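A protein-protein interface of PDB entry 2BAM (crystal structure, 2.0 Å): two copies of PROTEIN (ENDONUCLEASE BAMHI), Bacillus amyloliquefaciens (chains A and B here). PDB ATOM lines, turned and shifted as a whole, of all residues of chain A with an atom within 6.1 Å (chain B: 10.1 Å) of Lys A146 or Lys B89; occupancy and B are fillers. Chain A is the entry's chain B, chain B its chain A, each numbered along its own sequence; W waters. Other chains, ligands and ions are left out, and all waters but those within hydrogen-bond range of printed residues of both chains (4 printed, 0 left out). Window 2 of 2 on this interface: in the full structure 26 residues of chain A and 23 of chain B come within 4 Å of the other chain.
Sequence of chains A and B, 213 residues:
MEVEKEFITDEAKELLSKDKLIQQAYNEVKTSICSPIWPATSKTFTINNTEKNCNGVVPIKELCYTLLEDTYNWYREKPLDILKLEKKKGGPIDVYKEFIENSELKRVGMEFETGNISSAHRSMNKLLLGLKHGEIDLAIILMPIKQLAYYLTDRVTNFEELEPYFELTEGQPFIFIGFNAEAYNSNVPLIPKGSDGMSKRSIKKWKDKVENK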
ATOM      1  N   LYS A   5      -6.465  40.573 -33.010  1.00  0.00           N
ATOM      2  CA  LYS A   5      -5.772  40.495 -31.749  1.00  0.00           C
ATOM      3  C   LYS A   5      -4.480  41.258 -31.875  1.00  0.00           C
ATOM      4  O   LYS A   5      -3.900  41.363 -32.954  1.00  0.00           O
ATOM      5  CB  LYS A   5      -5.500  39.040 -31.367  1.00  0.00           C
ATOM      6  CG  LYS A   5      -6.743  38.200 -31.175  1.00  0.00           C
ATOM      7  CD  LYS A   5      -6.487  37.041 -30.251  1.00  0.00           C
ATOM      8  CE  LYS A   5      -7.791  36.348 -29.878  1.00  0.00           C
ATOM      9  NZ  LYS A   5      -8.481  35.775 -31.060  1.00  0.00           N
ATOM     10  N   PRO A 144      -1.484  35.065 -38.387  1.00  0.00           N
ATOM     11  CA  PRO A 144      -2.941  34.887 -38.366  1.00  0.00           C
ATOM     12  C   PRO A 144      -3.382  34.451 -36.984  1.00  0.00           C
ATOM     13  O   PRO A 144      -2.537  34.095 -36.157  1.00  0.00           O
ATOM     14  CB  PRO A 144      -3.158  33.774 -39.387  1.00  0.00           C
ATOM     15  CG  PRO A 144      -1.896  32.994 -39.298  1.00  0.00           C
ATOM     16  CD  PRO A 144      -0.845  34.063 -39.251  1.00  0.00           C
ATOM     17  N   ILE A 145      -4.686  34.528 -36.707  1.00  0.00           N
ATOM     18  CA  ILE A 145      -5.183  34.077 -35.414  1.00  0.00           C
ATOM     19  C   ILE A 145      -5.532  32.596 -35.555  1.00  0.00           C
ATOM     20  O   ILE A 145      -5.632  32.079 -36.670  1.00  0.00           O
ATOM     21  CB  ILE A 145      -6.421  34.873 -34.894  1.00  0.00           C
ATOM     22  CG1 ILE A 145      -7.597  34.776 -35.863  1.00  0.00           C
ATOM     23  CG2 ILE A 145      -6.058  36.306 -34.592  1.00  0.00           C
ATOM     24  CD1 ILE A 145      -8.860  35.347 -35.333  1.00  0.00           C
ATOM     25  N   LYS A 146      -5.728  31.936 -34.417  1.00  0.00           N
ATOM     26  CA  LYS A 146      -6.056  30.517 -34.345  1.00  0.00           C
ATOM     27  C   LYS A 146      -7.206  30.091 -35.272  1.00  0.00           C
ATOM     28  O   LYS A 146      -7.089  29.087 -35.976  1.00  0.00           O
ATOM     29  CB  LYS A 146      -6.380  30.163 -32.888  1.00  0.00           C
ATOM     30  CG  LYS A 146      -6.573  28.705 -32.582  1.00  0.00           C
ATOM     31  CD  LYS A 146      -6.515  28.500 -31.084  1.00  0.00           C
ATOM     32  CE  LYS A 146      -6.581  27.023 -30.714  1.00  0.00           C
ATOM     33  NZ  LYS A 146      -7.964  26.479 -30.881  1.00  0.00           N
ATOM     34  N   GLN A 147      -8.299  30.866 -35.288  1.00  0.00           N
ATOM     35  CA  GLN A 147      -9.455  30.541 -36.110  1.00  0.00           C
ATOM     36  C   GLN A 147      -9.127  30.520 -37.584  1.00  0.00           C
ATOM     37  O   GLN A 147      -9.664  29.710 -38.324  1.00  0.00           O
ATOM     38  CB  GLN A 147     -10.592  31.510 -35.861  1.00  0.00           C
ATOM     39  CG  GLN A 147     -11.809  31.199 -36.701  1.00  0.00           C
ATOM     40  CD  GLN A 147     -12.851  32.301 -36.694  1.00  0.00           C
ATOM     41  OE1 GLN A 147     -12.539  33.476 -36.454  1.00  0.00           O
ATOM     42  NE2 GLN A 147     -14.107  31.923 -36.955  1.00  0.00           N
ATOM     43  N   LEU A 148      -8.250  31.423 -38.021  1.00  0.00           N
ATOM     44  CA  LEU A 148      -7.859  31.476 -39.426  1.00  0.00           C
ATOM     45  C   LEU A 148      -6.885  30.346 -39.728  1.00  0.00           C
ATOM     46  O   LEU A 148      -7.034  29.626 -40.729  1.00  0.00           O
ATOM     47  CB  LEU A 148      -7.199  32.805 -39.754  1.00  0.00           C
ATOM     48  CG  LEU A 148      -6.704  32.984 -41.191  1.00  0.00           C
ATOM     49  CD1 LEU A 148      -7.772  32.557 -42.193  1.00  0.00           C
ATOM     50  CD2 LEU A 148      -6.337  34.431 -41.408  1.00  0.00           C
ATOM     51  N   ALA A 149      -5.907  30.188 -38.842  1.00  0.00           N
ATOM     52  CA  ALA A 149      -4.884  29.153 -38.957  1.00  0.00           C
ATOM     53  C   ALA A 149      -5.425  27.724 -38.952  1.00  0.00           C
ATOM     54  O   ALA A 149      -4.741  26.811 -39.386  1.00  0.00           O
ATOM     55  CB  ALA A 149      -3.830  29.345 -37.888  1.00  0.00           C
ATOM     56  N   TYR A 150      -6.649  27.538 -38.476  1.00  0.00           N
ATOM     57  CA  TYR A 150      -7.268  26.218 -38.466  1.00  0.00           C
ATOM     58  C   TYR A 150      -7.466  25.711 -39.903  1.00  0.00           C
ATOM     59  O   TYR A 150      -7.412  24.502 -40.183  1.00  0.00           O
ATOM     60  CB  TYR A 150      -8.626  26.255 -37.745  1.00  0.00           C
ATOM     61  CG  TYR A 150      -9.324  24.902 -37.715  1.00  0.00           C
ATOM     62  CD1 TYR A 150     -10.130  24.488 -38.779  1.00  0.00           C
ATOM     63  CD2 TYR A 150      -9.148  24.031 -36.643  1.00  0.00           C
ATOM     64  CE1 TYR A 150     -10.746  23.236 -38.777  1.00  0.00           C
ATOM     65  CE2 TYR A 150      -9.750  22.774 -36.632  1.00  0.00           C
ATOM     66  CZ  TYR A 150     -10.549  22.385 -37.696  1.00  0.00           C
ATOM     67  OH  TYR A 150     -11.159  21.153 -37.648  1.00  0.00           O
ATOM     68  N   TYR A 151      -7.676  26.654 -40.814  1.00  0.00           N
ATOM     69  CA  TYR A 151      -7.897  26.341 -42.204  1.00  0.00           C
ATOM     70  C   TYR A 151      -6.642  26.512 -43.044  1.00  0.00           C
ATOM     71  O   TYR A 151      -6.675  26.347 -44.268  1.00  0.00           O
ATOM     72  CB  TYR A 151      -9.050  27.185 -42.735  1.00  0.00           C
ATOM     73  CG  TYR A 151     -10.372  26.840 -42.075  1.00  0.00           C
ATOM     74  CD1 TYR A 151     -11.138  25.759 -42.516  1.00  0.00           C
ATOM     75  CD2 TYR A 151     -10.830  27.563 -40.976  1.00  0.00           C
ATOM     76  CE1 TYR A 151     -12.324  25.404 -41.875  1.00  0.00           C
ATOM     77  CE2 TYR A 151     -12.026  27.208 -40.325  1.00  0.00           C
ATOM     78  CZ  TYR A 151     -12.765  26.126 -40.784  1.00  0.00           C
ATOM     79  OH  TYR A 151     -13.940  25.765 -40.176  1.00  0.00           O
ATOM     80  N   ASN A 158       0.465  31.116 -35.070  1.00  0.00           N
ATOM     81  CA  ASN A 158      -0.848  31.679 -34.761  1.00  0.00           C
ATOM     82  C   ASN A 158      -0.746  32.503 -33.479  1.00  0.00           C
ATOM     83  O   ASN A 158       0.020  32.162 -32.572  1.00  0.00           O
ATOM     84  CB  ASN A 158      -1.917  30.582 -34.680  1.00  0.00           C
ATOM     85  CG  ASN A 158      -1.659  29.577 -33.588  1.00  0.00           C
ATOM     86  OD1 ASN A 158      -2.146  29.742 -32.471  1.00  0.00           O
ATOM     87  ND2 ASN A 158      -0.941  28.498 -33.915  1.00  0.00           N
ATOM     88  N   PHE A 159      -1.445  33.647 -33.456  1.00  0.00           N
ATOM     89  CA  PHE A 159      -1.393  34.583 -32.324  1.00  0.00           C
ATOM     90  C   PHE A 159      -1.485  33.947 -30.930  1.00  0.00           C
ATOM     91  O   PHE A 159      -0.633  34.183 -30.069  1.00  0.00           O
ATOM     92  CB  PHE A 159      -2.481  35.664 -32.477  1.00  0.00           C
ATOM     93  CG  PHE A 159      -2.334  36.816 -31.518  1.00  0.00           C
ATOM     94  CD1 PHE A 159      -2.893  36.762 -30.249  1.00  0.00           C
ATOM     95  CD2 PHE A 159      -1.613  37.946 -31.880  1.00  0.00           C
ATOM     96  CE1 PHE A 159      -2.730  37.815 -29.352  1.00  0.00           C
ATOM     97  CE2 PHE A 159      -1.443  39.007 -30.991  1.00  0.00           C
ATOM     98  CZ  PHE A 159      -2.007  38.933 -29.726  1.00  0.00           C
ATOM     99  N   GLU A 160      -2.521  33.148 -30.719  1.00  0.00           N
ATOM    100  CA  GLU A 160      -2.753  32.490 -29.445  1.00  0.00           C
ATOM    101  C   GLU A 160      -1.645  31.549 -28.989  1.00  0.00           C
ATOM    102  O   GLU A 160      -1.324  31.499 -27.793  1.00  0.00           O
ATOM    103  CB  GLU A 160      -4.108  31.774 -29.455  1.00  0.00           C
ATOM    104  CG  GLU A 160      -5.323  32.706 -29.600  1.00  0.00           C
ATOM    105  CD  GLU A 160      -5.751  32.968 -31.042  1.00  0.00           C
ATOM    106  OE1 GLU A 160      -6.941  33.252 -31.253  1.00  0.00           O
ATOM    107  OE2 GLU A 160      -4.925  32.884 -31.965  1.00  0.00           O
ATOM    108  N   GLU A 161      -1.024  30.842 -29.928  1.00  0.00           N
ATOM    109  CA  GLU A 161       0.039  29.918 -29.570  1.00  0.00           C
ATOM    110  C   GLU A 161       1.380  30.578 -29.235  1.00  0.00           C
ATOM    111  O   GLU A 161       2.194  30.000 -28.525  1.00  0.00           O
ATOM    112  CB  GLU A 161       0.209  28.844 -30.637  1.00  0.00           C
ATOM    113  CG  GLU A 161       1.102  27.728 -30.174  1.00  0.00           C
ATOM    114  CD  GLU A 161       0.954  26.435 -30.966  1.00  0.00           C
ATOM    115  OE1 GLU A 161       1.401  25.383 -30.449  1.00  0.00           O
ATOM    116  OE2 GLU A 161       0.403  26.478 -32.087  1.00  0.00           O
ATOM    117  N   PRO A 164       1.729  32.902 -25.006  1.00  0.00           N
ATOM    118  CA  PRO A 164       2.342  32.636 -23.698  1.00  0.00           C
ATOM    119  C   PRO A 164       3.759  33.212 -23.612  1.00  0.00           C
ATOM    120  O   PRO A 164       4.245  33.559 -22.539  1.00  0.00           O
ATOM    121  CB  PRO A 164       2.390  31.102 -23.635  1.00  0.00           C
ATOM    122  CG  PRO A 164       1.248  30.692 -24.466  1.00  0.00           C
ATOM    123  CD  PRO A 164       1.279  31.655 -25.637  1.00  0.00           C
ATOM    124  N   TYR A 165       4.393  33.363 -24.766  1.00  0.00           N
ATOM    125  CA  TYR A 165       5.752  33.858 -24.827  1.00  0.00           C
ATOM    126  C   TYR A 165       5.959  35.354 -25.098  1.00  0.00           C
ATOM    127  O   TYR A 165       7.088  35.810 -25.210  1.00  0.00           O
ATOM    128  CB  TYR A 165       6.533  33.002 -25.822  1.00  0.00           C
ATOM    129  CG  TYR A 165       6.456  31.520 -25.525  1.00  0.00           C
ATOM    130  CD1 TYR A 165       7.338  30.930 -24.634  1.00  0.00           C
ATOM    131  CD2 TYR A 165       5.511  30.712 -26.146  1.00  0.00           C
ATOM    132  CE1 TYR A 165       7.296  29.557 -24.360  1.00  0.00           C
ATOM    133  CE2 TYR A 165       5.457  29.333 -25.890  1.00  0.00           C
ATOM    134  CZ  TYR A 165       6.360  28.759 -24.992  1.00  0.00           C
ATOM    135  OH  TYR A 165       6.346  27.406 -24.747  1.00  0.00           O
ATOM    136  N   PHE A 179      -4.098  38.597 -37.327  1.00  0.00           N
ATOM    137  CA  PHE A 179      -5.094  38.888 -38.350  1.00  0.00           C
ATOM    138  C   PHE A 179      -6.044  37.732 -38.621  1.00  0.00           C
ATOM    139  O   PHE A 179      -5.726  36.579 -38.318  1.00  0.00           O
ATOM    140  CB  PHE A 179      -4.430  39.366 -39.653  1.00  0.00           C
ATOM    141  CG  PHE A 179      -3.524  38.347 -40.310  1.00  0.00           C
ATOM    142  CD1 PHE A 179      -4.034  37.404 -41.192  1.00  0.00           C
ATOM    143  CD2 PHE A 179      -2.148  38.376 -40.098  1.00  0.00           C
ATOM    144  CE1 PHE A 179      -3.188  36.510 -41.854  1.00  0.00           C
ATOM    145  CE2 PHE A 179      -1.298  37.489 -40.755  1.00  0.00           C
ATOM    146  CZ  PHE A 179      -1.824  36.552 -41.638  1.00  0.00           C
ATOM    147  N   PRO B  79       4.862  19.328 -17.203  1.00  0.00           N
ATOM    148  CA  PRO B  79       4.205  20.585 -17.563  1.00  0.00           C
ATOM    149  C   PRO B  79       4.588  21.686 -16.579  1.00  0.00           C
ATOM    150  O   PRO B  79       4.731  21.447 -15.384  1.00  0.00           O
ATOM    151  CB  PRO B  79       2.727  20.230 -17.445  1.00  0.00           C
ATOM    152  CG  PRO B  79       2.713  19.263 -16.314  1.00  0.00           C
ATOM    153  CD  PRO B  79       3.893  18.379 -16.621  1.00  0.00           C
ATOM    154  N   LEU B  80       4.832  22.882 -17.095  1.00  0.00           N
ATOM    155  CA  LEU B  80       5.173  24.011 -16.247  1.00  0.00           C
ATOM    156  C   LEU B  80       3.864  24.644 -15.782  1.00  0.00           C
ATOM    157  O   LEU B  80       2.872  24.624 -16.511  1.00  0.00           O
ATOM    158  CB  LEU B  80       5.992  25.044 -17.024  1.00  0.00           C
ATOM    159  CG  LEU B  80       7.373  24.639 -17.543  1.00  0.00           C
ATOM    160  CD1 LEU B  80       7.929  25.750 -18.410  1.00  0.00           C
ATOM    161  CD2 LEU B  80       8.310  24.348 -16.383  1.00  0.00           C
ATOM    162  N   ASP B  81       3.859  25.184 -14.567  1.00  0.00           N
ATOM    163  CA  ASP B  81       2.673  25.843 -14.009  1.00  0.00           C
ATOM    164  C   ASP B  81       2.278  27.081 -14.812  1.00  0.00           C
ATOM    165  O   ASP B  81       1.098  27.345 -15.045  1.00  0.00           O
ATOM    166  CB  ASP B  81       2.927  26.270 -12.561  1.00  0.00           C
ATOM    167  CG  ASP B  81       3.006  25.105 -11.605  1.00  0.00           C
ATOM    168  OD1 ASP B  81       3.448  25.321 -10.450  1.00  0.00           O
ATOM    169  OD2 ASP B  81       2.626  23.974 -11.988  1.00  0.00           O
ATOM    170  N   ILE B  82       3.277  27.864 -15.195  1.00  0.00           N
ATOM    171  CA  ILE B  82       3.029  29.063 -15.966  1.00  0.00           C
ATOM    172  C   ILE B  82       2.303  28.679 -17.247  1.00  0.00           C
ATOM    173  O   ILE B  82       1.324  29.326 -17.610  1.00  0.00           O
ATOM    174  CB  ILE B  82       4.354  29.846 -16.254  1.00  0.00           C
ATOM    175  CG1 ILE B  82       4.068  31.126 -17.040  1.00  0.00           C
ATOM    176  CG2 ILE B  82       5.369  28.974 -16.992  1.00  0.00           C
ATOM    177  CD1 ILE B  82       3.197  32.120 -16.300  1.00  0.00           C
ATOM    178  N   LEU B  83       2.695  27.561 -17.854  1.00  0.00           N
ATOM    179  CA  LEU B  83       2.065  27.122 -19.091  1.00  0.00           C
ATOM    180  C   LEU B  83       0.698  26.461 -19.003  1.00  0.00           C
ATOM    181  O   LEU B  83      -0.242  26.905 -19.658  1.00  0.00           O
ATOM    182  CB  LEU B  83       3.015  26.284 -19.936  1.00  0.00           C
ATOM    183  CG  LEU B  83       4.159  27.042 -20.606  1.00  0.00           C
ATOM    184  CD1 LEU B  83       4.723  26.152 -21.696  1.00  0.00           C
ATOM    185  CD2 LEU B  83       3.666  28.354 -21.202  1.00  0.00           C
ATOM    186  N   LYS B  84       0.556  25.388 -18.234  1.00  0.00           N
ATOM    187  CA  LYS B  84      -0.774  24.785 -18.187  1.00  0.00           C
ATOM    188  C   LYS B  84      -1.701  25.067 -17.011  1.00  0.00           C
ATOM    189  O   LYS B  84      -2.869  24.661 -17.034  1.00  0.00           O
ATOM    190  CB  LYS B  84      -0.761  23.303 -18.591  1.00  0.00           C
ATOM    191  CG  LYS B  84      -0.865  23.154 -20.130  1.00  0.00           C
ATOM    192  CD  LYS B  84      -1.628  21.914 -20.564  1.00  0.00           C
ATOM    193  CE  LYS B  84      -1.977  22.017 -22.059  1.00  0.00           C
ATOM    194  NZ  LYS B  84      -2.567  20.753 -22.600  1.00  0.00           N
ATOM    195  N   LEU B  85      -1.206  25.818 -16.031  1.00  0.00           N
ATOM    196  CA  LEU B  85      -2.014  26.191 -14.877  1.00  0.00           C
ATOM    197  C   LEU B  85      -2.504  27.621 -15.000  1.00  0.00           C
ATOM    198  O   LEU B  85      -3.698  27.864 -14.902  1.00  0.00           O
ATOM    199  CB  LEU B  85      -1.251  26.025 -13.561  1.00  0.00           C
ATOM    200  CG  LEU B  85      -1.073  24.618 -12.990  1.00  0.00           C
ATOM    201  CD1 LEU B  85      -0.639  24.741 -11.536  1.00  0.00           C
ATOM    202  CD2 LEU B  85      -2.374  23.836 -13.086  1.00  0.00           C
ATOM    203  N   GLU B  86      -1.582  28.562 -15.205  1.00  0.00           N
ATOM    204  CA  GLU B  86      -1.947  29.965 -15.333  1.00  0.00           C
ATOM    205  C   GLU B  86      -2.438  30.353 -16.721  1.00  0.00           C
ATOM    206  O   GLU B  86      -3.616  30.697 -16.904  1.00  0.00           O
ATOM    207  CB  GLU B  86      -0.777  30.860 -14.964  1.00  0.00           C
ATOM    208  CG  GLU B  86      -0.486  30.945 -13.482  1.00  0.00           C
ATOM    209  CD  GLU B  86       0.573  32.011 -13.144  1.00  0.00           C
ATOM    210  OE1 GLU B  86       0.893  32.864 -14.015  1.00  0.00           O
ATOM    211  OE2 GLU B  86       1.077  31.998 -11.995  1.00  0.00           O
ATOM    212  N   LYS B  87      -1.527  30.303 -17.694  1.00  0.00           N
ATOM    213  CA  LYS B  87      -1.842  30.676 -19.077  1.00  0.00           C
ATOM    214  C   LYS B  87      -2.678  29.669 -19.856  1.00  0.00           C
ATOM    215  O   LYS B  87      -3.280  30.015 -20.872  1.00  0.00           O
ATOM    216  CB  LYS B  87      -0.560  30.993 -19.849  1.00  0.00           C
ATOM    217  CG  LYS B  87       0.163  32.192 -19.304  1.00  0.00           C
ATOM    218  CD  LYS B  87       1.441  32.448 -20.030  1.00  0.00           C
ATOM    219  CE  LYS B  87       2.121  33.666 -19.454  1.00  0.00           C
ATOM    220  NZ  LYS B  87       3.453  33.878 -20.067  1.00  0.00           N
ATOM    221  N   LYS B  88      -2.705  28.426 -19.386  1.00  0.00           N
ATOM    222  CA  LYS B  88      -3.473  27.374 -20.032  1.00  0.00           C
ATOM    223  C   LYS B  88      -3.220  27.281 -21.537  1.00  0.00           C
ATOM    224  O   LYS B  88      -4.151  27.242 -22.353  1.00  0.00           O
ATOM    225  CB  LYS B  88      -4.961  27.561 -19.739  1.00  0.00           C
ATOM    226  CG  LYS B  88      -5.302  27.556 -18.251  1.00  0.00           C
ATOM    227  CD  LYS B  88      -6.783  27.293 -18.026  1.00  0.00           C
ATOM    228  CE  LYS B  88      -7.149  27.336 -16.545  1.00  0.00           C
ATOM    229  NZ  LYS B  88      -7.089  28.728 -16.000  1.00  0.00           N
ATOM    230  N   LYS B  89      -1.940  27.227 -21.889  1.00  0.00           N
ATOM    231  CA  LYS B  89      -1.505  27.142 -23.284  1.00  0.00           C
ATOM    232  C   LYS B  89      -0.062  26.633 -23.341  1.00  0.00           C
ATOM    233  O   LYS B  89       0.764  26.982 -22.479  1.00  0.00           O
ATOM    234  CB  LYS B  89      -1.605  28.517 -23.958  1.00  0.00           C
ATOM    235  CG  LYS B  89      -1.518  28.504 -25.472  1.00  0.00           C
ATOM    236  CD  LYS B  89      -2.712  27.848 -26.077  1.00  0.00           C
ATOM    237  CE  LYS B  89      -2.634  27.928 -27.593  1.00  0.00           C
ATOM    238  NZ  LYS B  89      -3.648  27.057 -28.261  1.00  0.00           N
ATOM    239  N   GLY B  90       0.226  25.804 -24.339  1.00  0.00           N
ATOM    240  CA  GLY B  90       1.562  25.261 -24.483  1.00  0.00           C
ATOM    241  C   GLY B  90       1.695  23.909 -23.819  1.00  0.00           C
ATOM    242  O   GLY B  90       0.891  23.558 -22.975  1.00  0.00           O
ATOM    243  N   GLY B  91       2.697  23.132 -24.240  1.00  0.00           N
ATOM    244  CA  GLY B  91       2.902  21.814 -23.666  1.00  0.00           C
ATOM    245  C   GLY B  91       4.022  21.796 -22.636  1.00  0.00           C
ATOM    246  O   GLY B  91       4.562  22.828 -22.298  1.00  0.00           O
ATOM    247  N   PRO B  92       4.404  20.603 -22.141  1.00  0.00           N
ATOM    248  CA  PRO B  92       5.430  20.397 -21.128  1.00  0.00           C
ATOM    249  C   PRO B  92       6.842  20.415 -21.683  1.00  0.00           C
ATOM    250  O   PRO B  92       7.062  20.471 -22.938  1.00  0.00           O
ATOM    251  CB  PRO B  92       5.127  19.030 -20.627  1.00  0.00           C
ATOM    252  CG  PRO B  92       4.678  18.334 -21.847  1.00  0.00           C
ATOM    253  CD  PRO B  92       3.775  19.336 -22.477  1.00  0.00           C
ATOM    254  N   ILE B  93       7.805  20.446 -20.762  1.00  0.00           N
ATOM    255  CA  ILE B  93       9.251  20.402 -21.181  1.00  0.00           C
ATOM    256  C   ILE B  93       9.625  18.913 -21.115  1.00  0.00           C
ATOM    257  O   ILE B  93       9.052  18.099 -20.436  1.00  0.00           O
ATOM    258  CB  ILE B  93      10.226  21.146 -20.191  1.00  0.00           C
ATOM    259  CG1 ILE B  93      10.087  20.667 -18.730  1.00  0.00           C
ATOM    260  CG2 ILE B  93       9.973  22.695 -20.257  1.00  0.00           C
ATOM    261  CD1 ILE B  93      11.053  21.367 -17.790  1.00  0.00           C
ATOM    262  N   ARG B 122      11.867  27.556 -29.369  1.00  0.00           N
ATOM    263  CA  ARG B 122      10.699  27.376 -28.504  1.00  0.00           C
ATOM    264  C   ARG B 122      11.151  26.738 -27.179  1.00  0.00           C
ATOM    265  O   ARG B 122      10.779  27.201 -26.084  1.00  0.00           O
ATOM    266  CB  ARG B 122       9.668  26.463 -29.188  1.00  0.00           C
ATOM    267  CG  ARG B 122       8.443  26.127 -28.321  1.00  0.00           C
ATOM    268  CD  ARG B 122       7.408  25.352 -29.075  1.00  0.00           C
ATOM    269  NE  ARG B 122       7.977  24.159 -29.689  1.00  0.00           N
ATOM    270  CZ  ARG B 122       7.544  23.616 -30.826  1.00  0.00           C
ATOM    271  NH1 ARG B 122       6.522  24.171 -31.460  1.00  0.00           N
ATOM    272  NH2 ARG B 122       8.159  22.552 -31.347  1.00  0.00           N
ATOM    273  N   LYS B 126      10.751  28.293 -23.554  1.00  0.00           N
ATOM    274  CA  LYS B 126       9.937  27.632 -22.535  1.00  0.00           C
ATOM    275  C   LYS B 126      10.718  27.512 -21.230  1.00  0.00           C
ATOM    276  O   LYS B 126      10.193  27.778 -20.157  1.00  0.00           O
ATOM    277  CB  LYS B 126       9.489  26.253 -23.012  1.00  0.00           C
ATOM    278  CG  LYS B 126       8.602  25.526 -22.049  1.00  0.00           C
ATOM    279  CD  LYS B 126       8.080  24.227 -22.633  1.00  0.00           C
ATOM    280  CE  LYS B 126       7.143  24.461 -23.802  1.00  0.00           C
ATOM    281  NZ  LYS B 126       6.731  23.179 -24.434  1.00  0.00           N
ATOM    282  N   LEU B 129      11.116  30.831 -19.665  1.00  0.00           N
ATOM    283  CA  LEU B 129       9.860  31.151 -19.022  1.00  0.00           C
ATOM    284  C   LEU B 129       9.841  30.445 -17.662  1.00  0.00           C
ATOM    285  O   LEU B 129       9.574  31.062 -16.638  1.00  0.00           O
ATOM    286  CB  LEU B 129       8.711  30.669 -19.910  1.00  0.00           C
ATOM    287  CG  LEU B 129       7.422  31.476 -20.057  1.00  0.00           C
ATOM    288  CD1 LEU B 129       7.716  32.922 -20.441  1.00  0.00           C
ATOM    289  CD2 LEU B 129       6.567  30.823 -21.113  1.00  0.00           C
ATOM    290  N   GLU B 135      10.282  28.179 -11.501  1.00  0.00           N
ATOM    291  CA  GLU B 135       9.886  26.774 -11.437  1.00  0.00           C
ATOM    292  C   GLU B 135      11.098  25.830 -11.521  1.00  0.00           C
ATOM    293  O   GLU B 135      11.071  24.716 -10.965  1.00  0.00           O
ATOM    294  CB  GLU B 135       8.832  26.459 -12.509  1.00  0.00           C
ATOM    295  CG  GLU B 135       7.512  27.189 -12.273  1.00  0.00           C
ATOM    296  CD  GLU B 135       6.430  26.784 -13.239  1.00  0.00           C
ATOM    297  OE1 GLU B 135       5.712  27.682 -13.736  1.00  0.00           O
ATOM    298  OE2 GLU B 135       6.279  25.560 -13.479  1.00  0.00           O
HETATM  299  O   HOH W   1       3.188  36.073 -22.570  1.00  0.00           O
HETATM  300  O   HOH W   2       4.182  25.473 -29.945  1.00  0.00           O
HETATM  301  O   HOH W   3       0.674  25.406 -27.693  1.00  0.00           O
HETATM  302  O   HOH W   4      -3.409  27.923 -31.031  1.00  0.00           O
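No position is printed for both chains.
Of the 10 pairs that touch across the chains among the printed residues, none has its exchanged pair printed and touching as well.
Among the printed residues, merely in contact across the chains: Lys A146 with Lys B89 (3.8 Å), Glu A160 with Lys B89 (3.8 Å), Glu A161 with Lys B89 (3.9 Å), Pro A164 with Leu B83 (3.9 Å), Pro A164 with Lys B89 (3.6 Å), Pro A164 with Leu B129 (3.9 Å), Tyr A165 with Leu B83 (3.7 Å), Tyr A165 with Lys B126 (3.2 Å) and Tyr A165 with Leu B129 (3.6 Å).
O of Ile B82 lies within hydrogen-bond range of N of Lys B87, at 3.0 Å.
The backbone carbonyl oxygen (O) of Leu B83 lies within hydrogen-bond range of the backbone NH (N) of Lys B88 (2.9 Å).
N of Lys B89 sits at hydrogen-bond distance from O of Leu B83 (2.8 Å).
NZ of Lys B126 sits at hydrogen-bond distance from O of Pro B92 (3.1 Å).
OE1 of Glu A160 lies within salt-bridge range of NZ of Lys A5 (3.0 Å).
The backbone NH (N) of Glu A161 is in hydrogen-bond range of the side-chain amide oxygen (OD1) of Asn A158 (3.0 Å).
Of the 19 printed residues of chain B, 5 touch a printed residue of chain A.
Among the printed residues, no Asp or Glu carboxylate lies within 4 Å of a Lys or Arg side-chain nitrogen of the other chain.
The backbone carbonyl oxygen (O) of Pro A164 is in hydrogen-bond range of the side-chain amino group (NZ) of Lys B87, at 2.6 Å.
No residue of chain B comes within 4 Å of Ile A145.
Of chain B, only Lys B89 (3.8 Å) comes within 4 Å of Lys A146.
No residue of chain B comes within 4 Å of Ala A149.
Glu A160 touches just one residue of chain B: Lys B89.
Glu A161 touches just one residue of chain B: Lys B89 (3.9 Å).
Printed residues of chain B within 4 Å of Tyr A165: Leu B83 (3.7 Å), Lys B126 (3.2 Å) and Leu B129 (3.6 Å).
Printed residues of chain A within 4 Å of Leu B83: Pro A164 and Tyr A165.
Of the printed residues of chain A, Lys B87 touches Pro A164 (2.6 Å).
Of the printed residues of chain A, Lys B89 touches Lys A146, Glu A160, Glu A161 and Pro A164.
Pro B92 touches none of the printed residues of chain A.
Of the printed residues of chain A, Leu B129 touches Pro A164 and Tyr A165.
The nearest residue of chain A that does not touch Lys B89 is Asn A158 (5.2 Å).
The nearest printed residue of chain A that does not touch Leu B129 is Glu A161 (8.6 Å).
Water W4 lies within hydrogen-bond range of the side-chain amide oxygen (OD1) of Asn A158 and the side-chain amino group (NZ) of Lys B89.
Water W1 bridges the backbone carbonyl oxygen (O) of Pro A164 (2.7 Å) and the side-chain amino group (NZ) of Lys B87 (3.3 Å).
Water W2 lies within hydrogen-bond range of OE1 of Glu A161 (2.8 Å) and NH1 of Arg B122 (3.1 Å).
Water W3 lies within hydrogen-bond range of the side-chain carboxylate (OE1) of Glu A161 (2.9 Å) and the backbone NH (N) of Gly B90 (3.4 Å).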
